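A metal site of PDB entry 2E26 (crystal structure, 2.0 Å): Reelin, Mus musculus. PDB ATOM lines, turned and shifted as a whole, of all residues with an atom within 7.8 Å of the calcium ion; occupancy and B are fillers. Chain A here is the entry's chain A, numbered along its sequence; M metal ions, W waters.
N of Asp 437 sits at hydrogen-bond distance from O of Asp 529 (3.0 Å). The side-chain carboxylate of Asp 382 sits at hydrogen-bond distance from the side-chain hydroxyl of Ser 384, 2.9 Å away.
The calcium ion is bound by O of Asp 382 (2.3 Å), water W1 (2.3 Å), O of Asp 408 (2.4 Å), O of Thr 406 (2.4 Å), water W2 (2.4 Å), OD1 of Asp 529 (2.5 Å) and OD2 of Asp 529 (2.5 Å).
Of the 19 residues printed, 4 come within 4 Å of the calcium ion.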
ATOM      1  N   ASP A 381     -18.044  19.251  -2.793  1.00  0.00           N
ATOM      2  CA  ASP A 381     -18.900  19.794  -1.758  1.00  0.00           C
ATOM      3  C   ASP A 381     -18.191  19.917  -0.412  1.00  0.00           C
ATOM      4  O   ASP A 381     -17.468  18.992   0.007  1.00  0.00           O
ATOM      5  CB  ASP A 381     -20.154  18.923  -1.580  1.00  0.00           C
ATOM      6  CG  ASP A 381     -21.413  19.746  -1.351  1.00  0.00           C
ATOM      7  OD1 ASP A 381     -22.438  19.374  -1.954  1.00  0.00           O
ATOM      8  OD2 ASP A 381     -21.380  20.750  -0.598  1.00  0.00           O
ATOM      9  N   ASP A 382     -18.383  21.057   0.256  1.00  0.00           N
ATOM     10  CA  ASP A 382     -17.940  21.255   1.639  1.00  0.00           C
ATOM     11  C   ASP A 382     -19.114  21.158   2.621  1.00  0.00           C
ATOM     12  O   ASP A 382     -18.955  21.331   3.835  1.00  0.00           O
ATOM     13  CB  ASP A 382     -17.229  22.609   1.787  1.00  0.00           C
ATOM     14  CG  ASP A 382     -18.154  23.810   1.549  1.00  0.00           C
ATOM     15  OD1 ASP A 382     -19.350  23.637   1.279  1.00  0.00           O
ATOM     16  OD2 ASP A 382     -17.654  24.954   1.630  1.00  0.00           O
ATOM     17  N   PHE A 383     -20.299  20.903   2.065  1.00  0.00           N
ATOM     18  CA  PHE A 383     -21.553  20.773   2.806  1.00  0.00           C
ATOM     19  C   PHE A 383     -22.000  22.000   3.587  1.00  0.00           C
ATOM     20  O   PHE A 383     -22.627  21.868   4.628  1.00  0.00           O
ATOM     21  CB  PHE A 383     -21.589  19.517   3.693  1.00  0.00           C
ATOM     22  CG  PHE A 383     -21.513  18.236   2.925  1.00  0.00           C
ATOM     23  CD1 PHE A 383     -22.595  17.817   2.142  1.00  0.00           C
ATOM     24  CD2 PHE A 383     -20.376  17.450   2.959  1.00  0.00           C
ATOM     25  CE1 PHE A 383     -22.536  16.637   1.412  1.00  0.00           C
ATOM     26  CE2 PHE A 383     -20.307  16.259   2.243  1.00  0.00           C
ATOM     27  CZ  PHE A 383     -21.402  15.849   1.476  1.00  0.00           C
ATOM     28  N   SER A 384     -21.651  23.180   3.059  1.00  0.00           N
ATOM     29  CA  SER A 384     -22.234  24.434   3.541  1.00  0.00           C
ATOM     30  C   SER A 384     -23.739  24.403   3.276  1.00  0.00           C
ATOM     31  O   SER A 384     -24.520  24.957   4.048  1.00  0.00           O
ATOM     32  CB  SER A 384     -21.572  25.651   2.877  1.00  0.00           C
ATOM     33  OG  SER A 384     -21.525  25.535   1.467  1.00  0.00           O
ATOM     34  N   THR A 385     -24.124  23.732   2.188  1.00  0.00           N
ATOM     35  CA  THR A 385     -25.520  23.448   1.869  1.00  0.00           C
ATOM     36  C   THR A 385     -25.619  21.971   1.511  1.00  0.00           C
ATOM     37  O   THR A 385     -24.599  21.316   1.247  1.00  0.00           O
ATOM     38  CB  THR A 385     -26.068  24.264   0.673  1.00  0.00           C
ATOM     39  OG1 THR A 385     -25.300  23.965  -0.508  1.00  0.00           O
ATOM     40  CG2 THR A 385     -26.032  25.761   0.957  1.00  0.00           C
ATOM     41  N   MET A 400     -24.800  18.847   9.384  1.00  0.00           N
ATOM     42  CA  MET A 400     -24.471  19.328  10.733  1.00  0.00           C
ATOM     43  C   MET A 400     -22.972  19.175  11.021  1.00  0.00           C
ATOM     44  O   MET A 400     -22.290  18.389  10.356  1.00  0.00           O
ATOM     45  CB  MET A 400     -25.287  18.562  11.786  1.00  0.00           C
ATOM     46  CG  MET A 400     -25.041  17.053  11.819  1.00  0.00           C
ATOM     47  SD  MET A 400     -26.061  16.215  13.054  1.00  0.00           S
ATOM     48  CE  MET A 400     -25.113  16.529  14.535  1.00  0.00           C
ATOM     49  N   PRO A 401     -22.455  19.920  12.009  1.00  0.00           N
ATOM     50  CA  PRO A 401     -21.079  19.656  12.450  1.00  0.00           C
ATOM     51  C   PRO A 401     -20.969  18.370  13.271  1.00  0.00           C
ATOM     52  O   PRO A 401     -21.944  17.945  13.910  1.00  0.00           O
ATOM     53  CB  PRO A 401     -20.745  20.875  13.316  1.00  0.00           C
ATOM     54  CG  PRO A 401     -22.062  21.356  13.824  1.00  0.00           C
ATOM     55  CD  PRO A 401     -23.074  21.041  12.757  1.00  0.00           C
ATOM     56  N   SER A 405     -15.496  19.178  12.797  1.00  0.00           N
ATOM     57  CA  SER A 405     -15.519  19.327  11.352  1.00  0.00           C
ATOM     58  C   SER A 405     -15.329  20.789  10.923  1.00  0.00           C
ATOM     59  O   SER A 405     -15.610  21.719  11.692  1.00  0.00           O
ATOM     60  CB  SER A 405     -16.821  18.765  10.774  1.00  0.00           C
ATOM     61  OG  SER A 405     -17.959  19.386  11.356  1.00  0.00           O
ATOM     62  N   THR A 406     -14.798  20.957   9.712  1.00  0.00           N
ATOM     63  CA  THR A 406     -14.711  22.271   9.092  1.00  0.00           C
ATOM     64  C   THR A 406     -16.111  22.619   8.577  1.00  0.00           C
ATOM     65  O   THR A 406     -16.578  22.047   7.586  1.00  0.00           O
ATOM     66  CB  THR A 406     -13.695  22.265   7.920  1.00  0.00           C
ATOM     67  OG1 THR A 406     -12.458  21.698   8.357  1.00  0.00           O
ATOM     68  CG2 THR A 406     -13.460  23.656   7.400  1.00  0.00           C
ATOM     69  N   GLY A 407     -16.780  23.528   9.266  1.00  0.00           N
ATOM     70  CA  GLY A 407     -18.188  23.811   8.998  1.00  0.00           C
ATOM     71  C   GLY A 407     -19.028  22.551   9.197  1.00  0.00           C
ATOM     72  O   GLY A 407     -18.650  21.640   9.951  1.00  0.00           O
ATOM     73  N   ASP A 408     -20.160  22.491   8.504  1.00  0.00           N
ATOM     74  CA  ASP A 408     -21.003  21.312   8.537  1.00  0.00           C
ATOM     75  C   ASP A 408     -20.425  20.174   7.684  1.00  0.00           C
ATOM     76  O   ASP A 408     -19.602  20.405   6.789  1.00  0.00           O
ATOM     77  CB  ASP A 408     -22.416  21.644   8.078  1.00  0.00           C
ATOM     78  CG  ASP A 408     -23.198  22.467   9.095  1.00  0.00           C
ATOM     79  OD1 ASP A 408     -22.661  22.764  10.188  1.00  0.00           O
ATOM     80  OD2 ASP A 408     -24.354  22.826   8.795  1.00  0.00           O
ATOM     81  N   ALA A 409     -20.874  18.967   7.989  1.00  0.00           N
ATOM     82  CA  ALA A 409     -20.547  17.752   7.255  1.00  0.00           C
ATOM     83  C   ALA A 409     -21.853  17.008   6.983  1.00  0.00           C
ATOM     84  O   ALA A 409     -22.911  17.419   7.477  1.00  0.00           O
ATOM     85  CB  ALA A 409     -19.625  16.890   8.083  1.00  0.00           C
ATOM     86  N   LEU A 410     -21.798  15.929   6.210  1.00  0.00           N
ATOM     87  CA  LEU A 410     -22.947  15.038   6.090  1.00  0.00           C
ATOM     88  C   LEU A 410     -22.767  13.891   7.088  1.00  0.00           C
ATOM     89  O   LEU A 410     -21.861  13.083   6.935  1.00  0.00           O
ATOM     90  CB  LEU A 410     -23.122  14.523   4.653  1.00  0.00           C
ATOM     91  CG  LEU A 410     -24.391  13.677   4.461  1.00  0.00           C
ATOM     92  CD1 LEU A 410     -25.688  14.524   4.587  1.00  0.00           C
ATOM     93  CD2 LEU A 410     -24.348  12.944   3.146  1.00  0.00           C
ATOM     94  N   ASP A 437     -12.887  13.617   3.070  1.00  0.00           N
ATOM     95  CA  ASP A 437     -12.593  13.458   4.486  1.00  0.00           C
ATOM     96  C   ASP A 437     -13.683  12.571   5.043  1.00  0.00           C
ATOM     97  O   ASP A 437     -14.865  12.714   4.678  1.00  0.00           O
ATOM     98  CB  ASP A 437     -12.583  14.805   5.223  1.00  0.00           C
ATOM     99  CG  ASP A 437     -11.384  15.685   4.854  1.00  0.00           C
ATOM    100  OD1 ASP A 437     -10.402  15.208   4.250  1.00  0.00           O
ATOM    101  OD2 ASP A 437     -11.427  16.866   5.202  1.00  0.00           O
ATOM    102  N   TRP A 494     -11.516  12.815  11.781  1.00  0.00           N
ATOM    103  CA  TRP A 494     -11.474  13.246  10.372  1.00  0.00           C
ATOM    104  C   TRP A 494     -10.149  12.898   9.705  1.00  0.00           C
ATOM    105  O   TRP A 494      -9.099  13.342  10.144  1.00  0.00           O
ATOM    106  CB  TRP A 494     -11.746  14.744  10.258  1.00  0.00           C
ATOM    107  CG  TRP A 494     -13.183  15.095  10.499  1.00  0.00           C
ATOM    108  CD1 TRP A 494     -13.703  15.729  11.592  1.00  0.00           C
ATOM    109  CD2 TRP A 494     -14.288  14.817   9.630  1.00  0.00           C
ATOM    110  NE1 TRP A 494     -15.065  15.866  11.449  1.00  0.00           N
ATOM    111  CE2 TRP A 494     -15.456  15.313  10.258  1.00  0.00           C
ATOM    112  CE3 TRP A 494     -14.417  14.187   8.374  1.00  0.00           C
ATOM    113  CZ2 TRP A 494     -16.716  15.203   9.685  1.00  0.00           C
ATOM    114  CZ3 TRP A 494     -15.684  14.090   7.801  1.00  0.00           C
ATOM    115  CH2 TRP A 494     -16.814  14.596   8.456  1.00  0.00           C
ATOM    116  N   ILE A 528     -19.069  12.337   6.279  1.00  0.00           N
ATOM    117  CA  ILE A 528     -18.187  12.728   5.169  1.00  0.00           C
ATOM    118  C   ILE A 528     -18.194  14.244   5.054  1.00  0.00           C
ATOM    119  O   ILE A 528     -19.188  14.902   5.420  1.00  0.00           O
ATOM    120  CB  ILE A 528     -18.577  12.061   3.805  1.00  0.00           C
ATOM    121  CG1 ILE A 528     -20.009  12.431   3.390  1.00  0.00           C
ATOM    122  CG2 ILE A 528     -18.425  10.522   3.862  1.00  0.00           C
ATOM    123  CD1 ILE A 528     -20.350  12.057   1.934  1.00  0.00           C
ATOM    124  N   ASP A 529     -17.085  14.809   4.577  1.00  0.00           N
ATOM    125  CA  ASP A 529     -16.933  16.240   4.340  1.00  0.00           C
ATOM    126  C   ASP A 529     -15.878  16.415   3.268  1.00  0.00           C
ATOM    127  O   ASP A 529     -15.200  15.440   2.888  1.00  0.00           O
ATOM    128  CB  ASP A 529     -16.497  16.962   5.631  1.00  0.00           C
ATOM    129  CG  ASP A 529     -16.778  18.469   5.591  1.00  0.00           C
ATOM    130  OD1 ASP A 529     -17.337  18.993   4.596  1.00  0.00           O
ATOM    131  OD2 ASP A 529     -16.457  19.152   6.583  1.00  0.00           O
ATOM    132  N   ASN A 530     -15.765  17.630   2.738  1.00  0.00           N
ATOM    133  CA  ASN A 530     -14.723  17.977   1.764  1.00  0.00           C
ATOM    134  C   ASN A 530     -14.568  16.971   0.629  1.00  0.00           C
ATOM    135  O   ASN A 530     -13.493  16.429   0.396  1.00  0.00           O
ATOM    136  CB  ASN A 530     -13.390  18.181   2.488  1.00  0.00           C
ATOM    137  CG  ASN A 530     -13.434  19.339   3.456  1.00  0.00           C
ATOM    138  OD1 ASN A 530     -14.075  20.363   3.185  1.00  0.00           O
ATOM    139  ND2 ASN A 530     -12.762  19.189   4.578  1.00  0.00           N
ATOM    140  N   VAL A 531     -15.666  16.723  -0.070  1.00  0.00           N
ATOM    141  CA  VAL A 531     -15.744  15.728  -1.111  1.00  0.00           C
ATOM    142  C   VAL A 531     -15.256  16.364  -2.395  1.00  0.00           C
ATOM    143  O   VAL A 531     -15.651  17.478  -2.741  1.00  0.00           O
ATOM    144  CB  VAL A 531     -17.203  15.269  -1.301  1.00  0.00           C
ATOM    145  CG1 VAL A 531     -17.395  14.389  -2.566  1.00  0.00           C
ATOM    146  CG2 VAL A 531     -17.693  14.554  -0.039  1.00  0.00           C
HETATM  147 CA    CA M   1     -17.666  21.165   5.681  1.00  0.00          CA
HETATM  148  O   HOH W   1     -15.629  21.773   4.759  1.00  0.00           O
HETATM  149  O   HOH W   2     -18.291  23.482   5.577  1.00  0.00           O
